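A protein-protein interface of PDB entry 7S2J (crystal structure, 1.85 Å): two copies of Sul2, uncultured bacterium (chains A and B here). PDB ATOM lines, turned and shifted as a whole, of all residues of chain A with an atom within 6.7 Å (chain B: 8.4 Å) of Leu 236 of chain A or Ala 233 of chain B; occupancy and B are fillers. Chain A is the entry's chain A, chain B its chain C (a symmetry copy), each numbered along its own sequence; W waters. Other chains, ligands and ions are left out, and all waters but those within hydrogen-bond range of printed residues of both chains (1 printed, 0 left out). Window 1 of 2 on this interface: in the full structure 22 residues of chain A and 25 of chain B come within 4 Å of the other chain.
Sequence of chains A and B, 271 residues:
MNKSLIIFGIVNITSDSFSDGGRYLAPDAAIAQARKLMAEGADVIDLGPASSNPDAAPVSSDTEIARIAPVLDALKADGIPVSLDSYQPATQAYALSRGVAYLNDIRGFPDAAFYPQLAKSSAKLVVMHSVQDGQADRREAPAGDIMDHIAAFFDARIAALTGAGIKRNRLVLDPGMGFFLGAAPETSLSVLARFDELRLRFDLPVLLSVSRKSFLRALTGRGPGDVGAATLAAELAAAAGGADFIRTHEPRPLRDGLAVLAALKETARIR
Of the 23 printed residues of chain B, 8 touch a printed residue of chain A. Hydrophobic or aromatic side chains of chain B within 4 Å of the printed part of chain A: Leu 192, Ala 229, Ala 230, Ala 233, Leu 236, Ala 237 and Leu 264. Of the 22 printed residues of chain A, 8 touch a printed residue of chain B. Hydrophobic or aromatic side chains of chain A that line the printed part of chain B: Leu 232, Ala 233, Leu 236, Ala 237, Pro 253, Val 260 and Leu 264. Among the printed residues, 10 pairs touch across the chains. Among the printed residues, no Asp or Glu carboxylate lies within 4 Å of a Lys or Arg side-chain nitrogen of the other chain.
Of chain B, only Ala 233 comes within 4 Å of Leu 236 of chain A. Ala 237 of chain A touches just one residue of chain B: Leu 264 (3.7 Å). Of the printed residues of chain B, Val 260 of chain A touches Ala 230 (3.7 Å) and Ala 234 (3.95 Å). Of the printed residues of chain A, Leu 236 of chain B touches Ala 233. The nearest residue of chain A that does not touch Ala 233 of chain B is Val 260 of chain A (4.1 Å). The nearest printed residue of chain B that does not touch Leu 232 of chain A is Leu 232 of chain B (4.2 Å).
Water W1 lies within hydrogen-bond range of N of Ala 230 of chain B, OD2 of Asp 256 of chain A and N of Ala 229 of chain B.
Leu 232 of chain A touches Ala 229 of chain B (CD2 to CB, 3.8 Å). Leu 236 of chain B touches Ala 233 of chain A. CB of Ala 233 of chain B touches CD1 of Leu 236 of chain A (3.8 Å). CB of Ala 237 of chain A touches CD1 of Leu 264 of chain B (3.7 Å). CA of Pro 253 of chain A touches CB of Ala 229 of chain B, 3.5 Å away. CA of Gly 257 of chain A touches CB of Ala 233 of chain B, at 3.6 Å. CG2 of Val 260 of chain A touches CB of Ala 230 of chain B, 3.7 Å away. Val 260 of chain A touches Ala 234 of chain B (CG1 to N, 3.95 Å). CG of Leu 192 of chain B touches CD2 of Leu 264 of chain A, 3.7 Å away. CD1 of Leu 264 of chain A touches CB of Ala 237 of chain B, at 3.7 Å.
Ala 233 of chain A touches Leu 236 of chain B, and with the chains exchanged Leu 236 of chain A touches Ala 233 of chain B. Ala 237 of chain A touches Leu 264 of chain B, and with the chains exchanged Leu 264 of chain A touches Ala 237 of chain B. Val 260 of chain A touches Ala 234 of chain B, but with the chains exchanged Ala 234 of chain A does not touch Val 260 of chain B (4.002 Å). Positions printed for both chains: 231, 232, 233, 234, 235, 236, 237, 238, 239, 240, 246, 253, 254, 260, 261 and 264. Of the 10 pairs that touch across the chains among the printed residues, 4 have their exchanged pair printed and touching as well.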
ATOM      1  N   THR A 231     -15.077 -10.596  27.381  1.00  0.00           N
ATOM      2  CA  THR A 231     -13.891 -11.129  28.038  1.00  0.00           C
ATOM      3  C   THR A 231     -12.773 -11.371  27.035  1.00  0.00           C
ATOM      4  O   THR A 231     -11.623 -10.981  27.259  1.00  0.00           O
ATOM      5  CB  THR A 231     -14.253 -12.429  28.759  1.00  0.00           C
ATOM      6  OG1 THR A 231     -15.124 -12.149  29.863  1.00  0.00           O
ATOM      7  CG2 THR A 231     -13.008 -13.150  29.228  1.00  0.00           C
ATOM      8  N   LEU A 232     -13.104 -12.001  25.902  1.00  0.00           N
ATOM      9  CA  LEU A 232     -12.084 -12.296  24.903  1.00  0.00           C
ATOM     10  C   LEU A 232     -11.453 -11.016  24.371  1.00  0.00           C
ATOM     11  O   LEU A 232     -10.230 -10.927  24.228  1.00  0.00           O
ATOM     12  CB  LEU A 232     -12.694 -13.113  23.754  1.00  0.00           C
ATOM     13  CG  LEU A 232     -11.707 -13.518  22.655  1.00  0.00           C
ATOM     14  CD1 LEU A 232     -10.467 -14.202  23.240  1.00  0.00           C
ATOM     15  CD2 LEU A 232     -12.386 -14.412  21.605  1.00  0.00           C
ATOM     16  N   ALA A 233     -12.278 -10.014  24.051  1.00  0.00           N
ATOM     17  CA  ALA A 233     -11.742  -8.743  23.582  1.00  0.00           C
ATOM     18  C   ALA A 233     -10.829  -8.112  24.628  1.00  0.00           C
ATOM     19  O   ALA A 233      -9.781  -7.550  24.293  1.00  0.00           O
ATOM     20  CB  ALA A 233     -12.889  -7.794  23.227  1.00  0.00           C
ATOM     21  N   ALA A 234     -11.215  -8.187  25.899  1.00  0.00           N
ATOM     22  CA  ALA A 234     -10.386  -7.599  26.951  1.00  0.00           C
ATOM     23  C   ALA A 234      -9.072  -8.357  27.103  1.00  0.00           C
ATOM     24  O   ALA A 234      -8.007  -7.745  27.259  1.00  0.00           O
ATOM     25  CB  ALA A 234     -11.152  -7.576  28.270  1.00  0.00           C
ATOM     26  N   GLU A 235      -9.124  -9.688  27.041  1.00  0.00           N
ATOM     27  CA  GLU A 235      -7.902 -10.475  27.146  1.00  0.00           C
ATOM     28  C   GLU A 235      -6.999 -10.253  25.944  1.00  0.00           C
ATOM     29  O   GLU A 235      -5.776 -10.156  26.097  1.00  0.00           O
ATOM     30  CB  GLU A 235      -8.249 -11.956  27.312  1.00  0.00           C
ATOM     31  CG  GLU A 235      -9.033 -12.209  28.594  1.00  0.00           C
ATOM     32  CD  GLU A 235      -9.546 -13.621  28.722  1.00  0.00           C
ATOM     33  OE1 GLU A 235      -9.791 -14.283  27.682  1.00  0.00           O
ATOM     34  OE2 GLU A 235      -9.725 -14.059  29.879  1.00  0.00           O
ATOM     35  N   LEU A 236      -7.580 -10.165  24.735  1.00  0.00           N
ATOM     36  CA  LEU A 236      -6.749  -9.931  23.555  1.00  0.00           C
ATOM     37  C   LEU A 236      -6.098  -8.551  23.602  1.00  0.00           C
ATOM     38  O   LEU A 236      -4.940  -8.395  23.203  1.00  0.00           O
ATOM     39  CB  LEU A 236      -7.582 -10.086  22.283  1.00  0.00           C
ATOM     40  CG  LEU A 236      -8.105 -11.507  22.017  1.00  0.00           C
ATOM     41  CD1 LEU A 236      -8.999 -11.525  20.775  1.00  0.00           C
ATOM     42  CD2 LEU A 236      -6.964 -12.507  21.861  1.00  0.00           C
ATOM     43  N   ALA A 237      -6.839  -7.534  24.058  1.00  0.00           N
ATOM     44  CA  ALA A 237      -6.260  -6.208  24.234  1.00  0.00           C
ATOM     45  C   ALA A 237      -5.134  -6.226  25.259  1.00  0.00           C
ATOM     46  O   ALA A 237      -4.110  -5.557  25.080  1.00  0.00           O
ATOM     47  CB  ALA A 237      -7.345  -5.216  24.652  1.00  0.00           C
ATOM     48  N   ALA A 238      -5.307  -6.975  26.350  1.00  0.00           N
ATOM     49  CA  ALA A 238      -4.227  -7.113  27.327  1.00  0.00           C
ATOM     50  C   ALA A 238      -3.015  -7.799  26.708  1.00  0.00           C
ATOM     51  O   ALA A 238      -1.873  -7.363  26.889  1.00  0.00           O
ATOM     52  CB  ALA A 238      -4.719  -7.888  28.550  1.00  0.00           C
ATOM     53  N   ALA A 239      -3.242  -8.878  25.966  1.00  0.00           N
ATOM     54  CA  ALA A 239      -2.127  -9.582  25.337  1.00  0.00           C
ATOM     55  C   ALA A 239      -1.375  -8.661  24.385  1.00  0.00           C
ATOM     56  O   ALA A 239      -0.141  -8.604  24.404  1.00  0.00           O
ATOM     57  CB  ALA A 239      -2.646 -10.823  24.601  1.00  0.00           C
ATOM     58  N   ALA A 240      -2.114  -7.920  23.551  1.00  0.00           N
ATOM     59  CA  ALA A 240      -1.487  -7.002  22.605  1.00  0.00           C
ATOM     60  C   ALA A 240      -0.754  -5.874  23.316  1.00  0.00           C
ATOM     61  O   ALA A 240       0.263  -5.381  22.812  1.00  0.00           O
ATOM     62  CB  ALA A 240      -2.539  -6.441  21.650  1.00  0.00           C
ATOM     63  N   GLY A 241      -1.250  -5.451  24.476  1.00  0.00           N
ATOM     64  CA  GLY A 241      -0.567  -4.483  25.310  1.00  0.00           C
ATOM     65  C   GLY A 241       0.627  -5.010  26.081  1.00  0.00           C
ATOM     66  O   GLY A 241       1.296  -4.234  26.765  1.00  0.00           O
ATOM     67  N   ILE A 246      -2.249 -14.358  31.603  1.00  0.00           N
ATOM     68  CA  ILE A 246      -3.669 -14.065  31.697  1.00  0.00           C
ATOM     69  C   ILE A 246      -4.328 -15.231  32.416  1.00  0.00           C
ATOM     70  O   ILE A 246      -4.092 -16.395  32.069  1.00  0.00           O
ATOM     71  CB  ILE A 246      -4.302 -13.816  30.313  1.00  0.00           C
ATOM     72  CG1 ILE A 246      -3.701 -12.555  29.692  1.00  0.00           C
ATOM     73  CG2 ILE A 246      -5.814 -13.658  30.431  1.00  0.00           C
ATOM     74  CD1 ILE A 246      -4.317 -12.195  28.348  1.00  0.00           C
ATOM     75  N   PRO A 253     -11.025 -20.051  23.735  1.00  0.00           N
ATOM     76  CA  PRO A 253     -11.245 -18.842  22.923  1.00  0.00           C
ATOM     77  C   PRO A 253     -10.040 -17.919  22.917  1.00  0.00           C
ATOM     78  O   PRO A 253      -9.707 -17.322  21.885  1.00  0.00           O
ATOM     79  CB  PRO A 253     -12.454 -18.178  23.601  1.00  0.00           C
ATOM     80  CG  PRO A 253     -13.143 -19.275  24.321  1.00  0.00           C
ATOM     81  CD  PRO A 253     -12.061 -20.198  24.776  1.00  0.00           C
ATOM     82  N   LEU A 254      -9.357 -17.807  24.057  1.00  0.00           N
ATOM     83  CA  LEU A 254      -8.168 -16.967  24.120  1.00  0.00           C
ATOM     84  C   LEU A 254      -7.047 -17.561  23.277  1.00  0.00           C
ATOM     85  O   LEU A 254      -6.375 -16.849  22.522  1.00  0.00           O
ATOM     86  CB  LEU A 254      -7.730 -16.794  25.583  1.00  0.00           C
ATOM     87  CG  LEU A 254      -6.440 -15.994  25.818  1.00  0.00           C
ATOM     88  CD1 LEU A 254      -6.540 -14.598  25.182  1.00  0.00           C
ATOM     89  CD2 LEU A 254      -6.153 -15.876  27.313  1.00  0.00           C
ATOM     90  N   ARG A 255      -6.823 -18.867  23.405  1.00  0.00           N
ATOM     91  CA  ARG A 255      -5.820 -19.530  22.583  1.00  0.00           C
ATOM     92  C   ARG A 255      -6.095 -19.298  21.097  1.00  0.00           C
ATOM     93  O   ARG A 255      -5.198 -18.914  20.337  1.00  0.00           O
ATOM     94  CB  ARG A 255      -5.801 -21.022  22.925  1.00  0.00           C
ATOM     95  CG  ARG A 255      -4.513 -21.734  22.593  1.00  0.00           C
ATOM     96  CD  ARG A 255      -3.343 -20.785  22.666  1.00  0.00           C
ATOM     97  NE  ARG A 255      -2.741 -20.670  23.987  1.00  0.00           N
ATOM     98  CZ  ARG A 255      -1.686 -19.912  24.248  1.00  0.00           C
ATOM     99  NH1 ARG A 255      -1.111 -19.180  23.307  1.00  0.00           N
ATOM    100  NH2 ARG A 255      -1.192 -19.888  25.483  1.00  0.00           N
ATOM    101  N   ASP A 256      -7.343 -19.511  20.668  1.00  0.00           N
ATOM    102  CA  ASP A 256      -7.693 -19.291  19.264  1.00  0.00           C
ATOM    103  C   ASP A 256      -7.487 -17.835  18.850  1.00  0.00           C
ATOM    104  O   ASP A 256      -6.926 -17.560  17.784  1.00  0.00           O
ATOM    105  CB  ASP A 256      -9.141 -19.699  19.002  1.00  0.00           C
ATOM    106  CG  ASP A 256      -9.385 -21.174  19.221  1.00  0.00           C
ATOM    107  OD1 ASP A 256      -8.404 -21.934  19.348  1.00  0.00           O
ATOM    108  OD2 ASP A 256     -10.566 -21.579  19.229  1.00  0.00           O
ATOM    109  N   GLY A 257      -7.963 -16.891  19.664  1.00  0.00           N
ATOM    110  CA  GLY A 257      -7.787 -15.485  19.334  1.00  0.00           C
ATOM    111  C   GLY A 257      -6.328 -15.089  19.219  1.00  0.00           C
ATOM    112  O   GLY A 257      -5.944 -14.367  18.296  1.00  0.00           O
ATOM    113  N   LEU A 258      -5.491 -15.579  20.140  1.00  0.00           N
ATOM    114  CA  LEU A 258      -4.060 -15.278  20.099  1.00  0.00           C
ATOM    115  C   LEU A 258      -3.411 -15.841  18.842  1.00  0.00           C
ATOM    116  O   LEU A 258      -2.514 -15.215  18.261  1.00  0.00           O
ATOM    117  CB  LEU A 258      -3.374 -15.833  21.353  1.00  0.00           C
ATOM    118  CG  LEU A 258      -3.753 -15.129  22.665  1.00  0.00           C
ATOM    119  CD1 LEU A 258      -3.196 -15.888  23.890  1.00  0.00           C
ATOM    120  CD2 LEU A 258      -3.265 -13.698  22.662  1.00  0.00           C
ATOM    121  N   ALA A 259      -3.849 -17.031  18.414  1.00  0.00           N
ATOM    122  CA  ALA A 259      -3.307 -17.641  17.204  1.00  0.00           C
ATOM    123  C   ALA A 259      -3.597 -16.789  15.976  1.00  0.00           C
ATOM    124  O   ALA A 259      -2.761 -16.691  15.066  1.00  0.00           O
ATOM    125  CB  ALA A 259      -3.872 -19.053  17.027  1.00  0.00           C
ATOM    126  N   VAL A 260      -4.778 -16.165  15.923  1.00  0.00           N
ATOM    127  CA  VAL A 260      -5.088 -15.284  14.799  1.00  0.00           C
ATOM    128  C   VAL A 260      -4.173 -14.062  14.826  1.00  0.00           C
ATOM    129  O   VAL A 260      -3.572 -13.692  13.808  1.00  0.00           O
ATOM    130  CB  VAL A 260      -6.581 -14.895  14.821  1.00  0.00           C
ATOM    131  CG1 VAL A 260      -6.860 -13.727  13.890  1.00  0.00           C
ATOM    132  CG2 VAL A 260      -7.448 -16.111  14.457  1.00  0.00           C
ATOM    133  N   LEU A 261      -4.042 -13.426  15.996  1.00  0.00           N
ATOM    134  CA  LEU A 261      -3.169 -12.259  16.109  1.00  0.00           C
ATOM    135  C   LEU A 261      -1.725 -12.614  15.772  1.00  0.00           C
ATOM    136  O   LEU A 261      -1.060 -11.895  15.014  1.00  0.00           O
ATOM    137  CB  LEU A 261      -3.263 -11.654  17.512  1.00  0.00           C
ATOM    138  CG  LEU A 261      -4.636 -11.110  17.915  1.00  0.00           C
ATOM    139  CD1 LEU A 261      -4.541 -10.273  19.172  1.00  0.00           C
ATOM    140  CD2 LEU A 261      -5.233 -10.306  16.778  1.00  0.00           C
ATOM    141  N   LEU A 264      -1.298 -12.926  12.106  1.00  0.00           N
ATOM    142  CA  LEU A 264      -1.376 -11.659  11.388  1.00  0.00           C
ATOM    143  C   LEU A 264      -0.056 -10.898  11.445  1.00  0.00           C
ATOM    144  O   LEU A 264       0.393 -10.349  10.431  1.00  0.00           O
ATOM    145  CB  LEU A 264      -2.495 -10.805  11.964  1.00  0.00           C
ATOM    146  CG  LEU A 264      -3.910 -11.074  11.465  1.00  0.00           C
ATOM    147  CD1 LEU A 264      -4.878 -10.226  12.272  1.00  0.00           C
ATOM    148  CD2 LEU A 264      -4.019 -10.743   9.992  1.00  0.00           C
ATOM    149  N   LEU B 192      -6.151  -9.330   5.229  1.00  0.00           N
ATOM    150  CA  LEU B 192      -6.615  -8.904   6.545  1.00  0.00           C
ATOM    151  C   LEU B 192      -5.603  -7.999   7.240  1.00  0.00           C
ATOM    152  O   LEU B 192      -5.992  -7.079   7.970  1.00  0.00           O
ATOM    153  CB  LEU B 192      -6.923 -10.126   7.404  1.00  0.00           C
ATOM    154  CG  LEU B 192      -7.428  -9.854   8.821  1.00  0.00           C
ATOM    155  CD1 LEU B 192      -8.626  -8.915   8.813  1.00  0.00           C
ATOM    156  CD2 LEU B 192      -7.772 -11.172   9.503  1.00  0.00           C
ATOM    157  N   VAL B 210     -14.704 -11.644   7.061  1.00  0.00           N
ATOM    158  CA  VAL B 210     -13.922 -12.820   7.428  1.00  0.00           C
ATOM    159  C   VAL B 210     -14.783 -13.884   8.075  1.00  0.00           C
ATOM    160  O   VAL B 210     -14.335 -15.036   8.190  1.00  0.00           O
ATOM    161  CB  VAL B 210     -12.754 -12.458   8.376  1.00  0.00           C
ATOM    162  CG1 VAL B 210     -11.813 -11.474   7.716  1.00  0.00           C
ATOM    163  CG2 VAL B 210     -13.288 -11.874   9.669  1.00  0.00           C
ATOM    164  N   LEU B 216      -9.748 -19.483   8.692  1.00  0.00           N
ATOM    165  CA  LEU B 216      -9.627 -19.372  10.143  1.00  0.00           C
ATOM    166  C   LEU B 216      -9.491 -20.739  10.792  1.00  0.00           C
ATOM    167  O   LEU B 216      -8.870 -20.863  11.852  1.00  0.00           O
ATOM    168  CB  LEU B 216     -10.842 -18.651  10.725  1.00  0.00           C
ATOM    169  CG  LEU B 216     -11.077 -17.204  10.278  1.00  0.00           C
ATOM    170  CD1 LEU B 216     -12.434 -16.716  10.763  1.00  0.00           C
ATOM    171  CD2 LEU B 216      -9.967 -16.286  10.750  1.00  0.00           C
ATOM    172  N   VAL B 227     -15.180 -21.975  15.458  1.00  0.00           N
ATOM    173  CA  VAL B 227     -14.462 -20.865  14.835  1.00  0.00           C
ATOM    174  C   VAL B 227     -14.920 -19.509  15.339  1.00  0.00           C
ATOM    175  O   VAL B 227     -14.443 -18.483  14.827  1.00  0.00           O
ATOM    176  CB  VAL B 227     -14.585 -20.905  13.300  1.00  0.00           C
ATOM    177  CG1 VAL B 227     -13.565 -21.870  12.700  1.00  0.00           C
ATOM    178  CG2 VAL B 227     -16.010 -21.245  12.891  1.00  0.00           C
ATOM    179  N   GLY B 228     -15.844 -19.463  16.301  1.00  0.00           N
ATOM    180  CA  GLY B 228     -16.392 -18.182  16.722  1.00  0.00           C
ATOM    181  C   GLY B 228     -15.358 -17.273  17.360  1.00  0.00           C
ATOM    182  O   GLY B 228     -15.376 -16.056  17.150  1.00  0.00           O
ATOM    183  N   ALA B 229     -14.442 -17.845  18.147  1.00  0.00           N
ATOM    184  CA  ALA B 229     -13.441 -17.011  18.816  1.00  0.00           C
ATOM    185  C   ALA B 229     -12.419 -16.481  17.819  1.00  0.00           C
ATOM    186  O   ALA B 229     -12.047 -15.301  17.870  1.00  0.00           O
ATOM    187  CB  ALA B 229     -12.750 -17.795  19.928  1.00  0.00           C
ATOM    188  N   ALA B 230     -11.962 -17.335  16.902  1.00  0.00           N
ATOM    189  CA  ALA B 230     -11.052 -16.882  15.856  1.00  0.00           C
ATOM    190  C   ALA B 230     -11.704 -15.815  14.985  1.00  0.00           C
ATOM    191  O   ALA B 230     -11.056 -14.837  14.603  1.00  0.00           O
ATOM    192  CB  ALA B 230     -10.593 -18.067  15.004  1.00  0.00           C
ATOM    193  N   THR B 231     -12.985 -15.993  14.646  1.00  0.00           N
ATOM    194  CA  THR B 231     -13.710 -14.976  13.885  1.00  0.00           C
ATOM    195  C   THR B 231     -13.708 -13.634  14.613  1.00  0.00           C
ATOM    196  O   THR B 231     -13.408 -12.590  14.019  1.00  0.00           O
ATOM    197  CB  THR B 231     -15.143 -15.442  13.625  1.00  0.00           C
ATOM    198  OG1 THR B 231     -15.116 -16.536  12.700  1.00  0.00           O
ATOM    199  CG2 THR B 231     -15.992 -14.315  13.055  1.00  0.00           C
ATOM    200  N   LEU B 232     -14.041 -13.641  15.906  1.00  0.00           N
ATOM    201  CA  LEU B 232     -14.086 -12.380  16.643  1.00  0.00           C
ATOM    202  C   LEU B 232     -12.722 -11.702  16.648  1.00  0.00           C
ATOM    203  O   LEU B 232     -12.628 -10.487  16.426  1.00  0.00           O
ATOM    204  CB  LEU B 232     -14.583 -12.603  18.069  1.00  0.00           C
ATOM    205  CG  LEU B 232     -14.703 -11.347  18.945  1.00  0.00           C
ATOM    206  CD1 LEU B 232     -15.545 -10.248  18.273  1.00  0.00           C
ATOM    207  CD2 LEU B 232     -15.273 -11.694  20.312  1.00  0.00           C
ATOM    208  N   ALA B 233     -11.653 -12.472  16.894  1.00  0.00           N
ATOM    209  CA  ALA B 233     -10.312 -11.891  16.909  1.00  0.00           C
ATOM    210  C   ALA B 233      -9.962 -11.268  15.569  1.00  0.00           C
ATOM    211  O   ALA B 233      -9.348 -10.199  15.516  1.00  0.00           O
ATOM    212  CB  ALA B 233      -9.275 -12.948  17.277  1.00  0.00           C
ATOM    213  N   ALA B 234     -10.332 -11.930  14.469  1.00  0.00           N
ATOM    214  CA  ALA B 234     -10.031 -11.370  13.159  1.00  0.00           C
ATOM    215  C   ALA B 234     -10.850 -10.108  12.911  1.00  0.00           C
ATOM    216  O   ALA B 234     -10.335  -9.133  12.361  1.00  0.00           O
ATOM    217  CB  ALA B 234     -10.288 -12.411  12.076  1.00  0.00           C
ATOM    218  N   GLU B 235     -12.115 -10.097  13.342  1.00  0.00           N
ATOM    219  CA  GLU B 235     -12.958  -8.917  13.142  1.00  0.00           C
ATOM    220  C   GLU B 235     -12.505  -7.750  14.014  1.00  0.00           C
ATOM    221  O   GLU B 235     -12.528  -6.593  13.572  1.00  0.00           O
ATOM    222  CB  GLU B 235     -14.424  -9.264  13.414  1.00  0.00           C
ATOM    223  CG  GLU B 235     -15.018 -10.220  12.366  1.00  0.00           C
ATOM    224  CD  GLU B 235     -16.367 -10.798  12.756  1.00  0.00           C
ATOM    225  OE1 GLU B 235     -16.732 -10.744  13.947  1.00  0.00           O
ATOM    226  OE2 GLU B 235     -17.069 -11.313  11.857  1.00  0.00           O
ATOM    227  N   LEU B 236     -12.094  -8.028  15.251  1.00  0.00           N
ATOM    228  CA  LEU B 236     -11.555  -6.963  16.087  1.00  0.00           C
ATOM    229  C   LEU B 236     -10.257  -6.430  15.511  1.00  0.00           C
ATOM    230  O   LEU B 236     -10.007  -5.222  15.544  1.00  0.00           O
ATOM    231  CB  LEU B 236     -11.350  -7.466  17.516  1.00  0.00           C
ATOM    232  CG  LEU B 236     -12.655  -7.703  18.281  1.00  0.00           C
ATOM    233  CD1 LEU B 236     -12.374  -8.320  19.668  1.00  0.00           C
ATOM    234  CD2 LEU B 236     -13.442  -6.391  18.396  1.00  0.00           C
ATOM    235  N   ALA B 237      -9.418  -7.319  14.972  1.00  0.00           N
ATOM    236  CA  ALA B 237      -8.204  -6.866  14.308  1.00  0.00           C
ATOM    237  C   ALA B 237      -8.533  -5.992  13.103  1.00  0.00           C
ATOM    238  O   ALA B 237      -7.889  -4.961  12.882  1.00  0.00           O
ATOM    239  CB  ALA B 237      -7.354  -8.067  13.894  1.00  0.00           C
ATOM    240  N   ALA B 238      -9.535  -6.384  12.311  1.00  0.00           N
ATOM    241  CA  ALA B 238      -9.942  -5.546  11.183  1.00  0.00           C
ATOM    242  C   ALA B 238     -10.420  -4.178  11.661  1.00  0.00           C
ATOM    243  O   ALA B 238     -10.051  -3.146  11.091  1.00  0.00           O
ATOM    244  CB  ALA B 238     -11.038  -6.247  10.372  1.00  0.00           C
ATOM    245  N   ALA B 239     -11.238  -4.153  12.714  1.00  0.00           N
ATOM    246  CA  ALA B 239     -11.700  -2.889  13.272  1.00  0.00           C
ATOM    247  C   ALA B 239     -10.529  -2.026  13.715  1.00  0.00           C
ATOM    248  O   ALA B 239     -10.470  -0.834  13.402  1.00  0.00           O
ATOM    249  CB  ALA B 239     -12.637  -3.151  14.449  1.00  0.00           C
ATOM    250  N   ALA B 240      -9.591  -2.614  14.460  1.00  0.00           N
ATOM    251  CA  ALA B 240      -8.421  -1.866  14.906  1.00  0.00           C
ATOM    252  C   ALA B 240      -7.584  -1.398  13.728  1.00  0.00           C
ATOM    253  O   ALA B 240      -6.933  -0.348  13.804  1.00  0.00           O
ATOM    254  CB  ALA B 240      -7.576  -2.720  15.853  1.00  0.00           C
ATOM    255  N   ILE B 246     -17.855  -4.129   8.455  1.00  0.00           N
ATOM    256  CA  ILE B 246     -17.566  -5.537   8.688  1.00  0.00           C
ATOM    257  C   ILE B 246     -18.856  -6.309   8.459  1.00  0.00           C
ATOM    258  O   ILE B 246     -19.915  -5.917   8.960  1.00  0.00           O
ATOM    259  CB  ILE B 246     -17.006  -5.809  10.100  1.00  0.00           C
ATOM    260  CG1 ILE B 246     -15.627  -5.148  10.244  1.00  0.00           C
ATOM    261  CG2 ILE B 246     -16.955  -7.319  10.351  1.00  0.00           C
ATOM    262  CD1 ILE B 246     -14.902  -5.450  11.551  1.00  0.00           C
ATOM    263  N   PRO B 253     -21.361 -10.577  19.430  1.00  0.00           N
ATOM    264  CA  PRO B 253     -20.000 -10.630  19.979  1.00  0.00           C
ATOM    265  C   PRO B 253     -19.123  -9.507  19.466  1.00  0.00           C
ATOM    266  O   PRO B 253     -18.265  -9.003  20.203  1.00  0.00           O
ATOM    267  CB  PRO B 253     -19.482 -11.999  19.511  1.00  0.00           C
ATOM    268  CG  PRO B 253     -20.688 -12.782  19.183  1.00  0.00           C
ATOM    269  CD  PRO B 253     -21.679 -11.799  18.668  1.00  0.00           C
ATOM    270  N   LEU B 254     -19.328  -9.091  18.217  1.00  0.00           N
ATOM    271  CA  LEU B 254     -18.511  -8.028  17.653  1.00  0.00           C
ATOM    272  C   LEU B 254     -18.847  -6.681  18.291  1.00  0.00           C
ATOM    273  O   LEU B 254     -17.936  -5.913  18.628  1.00  0.00           O
ATOM    274  CB  LEU B 254     -18.693  -7.992  16.132  1.00  0.00           C
ATOM    275  CG  LEU B 254     -17.953  -6.906  15.347  1.00  0.00           C
ATOM    276  CD1 LEU B 254     -16.450  -7.029  15.581  1.00  0.00           C
ATOM    277  CD2 LEU B 254     -18.292  -6.989  13.862  1.00  0.00           C
ATOM    278  N   VAL B 260     -15.661  -2.817  24.292  1.00  0.00           N
ATOM    279  CA  VAL B 260     -14.482  -2.907  25.150  1.00  0.00           C
ATOM    280  C   VAL B 260     -13.342  -2.088  24.564  1.00  0.00           C
ATOM    281  O   VAL B 260     -12.700  -1.298  25.265  1.00  0.00           O
ATOM    282  CB  VAL B 260     -14.065  -4.376  25.345  1.00  0.00           C
ATOM    283  CG1 VAL B 260     -12.651  -4.452  25.933  1.00  0.00           C
ATOM    284  CG2 VAL B 260     -15.068  -5.107  26.209  1.00  0.00           C
ATOM    285  N   LEU B 261     -13.073  -2.257  23.268  1.00  0.00           N
ATOM    286  CA  LEU B 261     -11.985  -1.507  22.648  1.00  0.00           C
ATOM    287  C   LEU B 261     -12.257  -0.004  22.663  1.00  0.00           C
ATOM    288  O   LEU B 261     -11.324   0.795  22.816  1.00  0.00           O
ATOM    289  CB  LEU B 261     -11.742  -1.992  21.214  1.00  0.00           C
ATOM    290  CG  LEU B 261     -11.337  -3.458  21.013  1.00  0.00           C
ATOM    291  CD1 LEU B 261     -10.779  -3.648  19.611  1.00  0.00           C
ATOM    292  CD2 LEU B 261     -10.350  -3.947  22.076  1.00  0.00           C
ATOM    293  N   LEU B 264     -11.581   1.311  26.201  1.00  0.00           N
ATOM    294  CA  LEU B 264     -10.140   1.353  26.422  1.00  0.00           C
ATOM    295  C   LEU B 264      -9.508   2.542  25.709  1.00  0.00           C
ATOM    296  O   LEU B 264      -8.650   3.229  26.275  1.00  0.00           O
ATOM    297  CB  LEU B 264      -9.503   0.046  25.945  1.00  0.00           C
ATOM    298  CG  LEU B 264      -9.711  -1.158  26.863  1.00  0.00           C
ATOM    299  CD1 LEU B 264      -9.165  -2.419  26.220  1.00  0.00           C
ATOM    300  CD2 LEU B 264      -9.055  -0.900  28.227  1.00  0.00           C
HETATM  301  O   HOH W   1     -12.257 -20.169  17.294  1.00  0.00           O
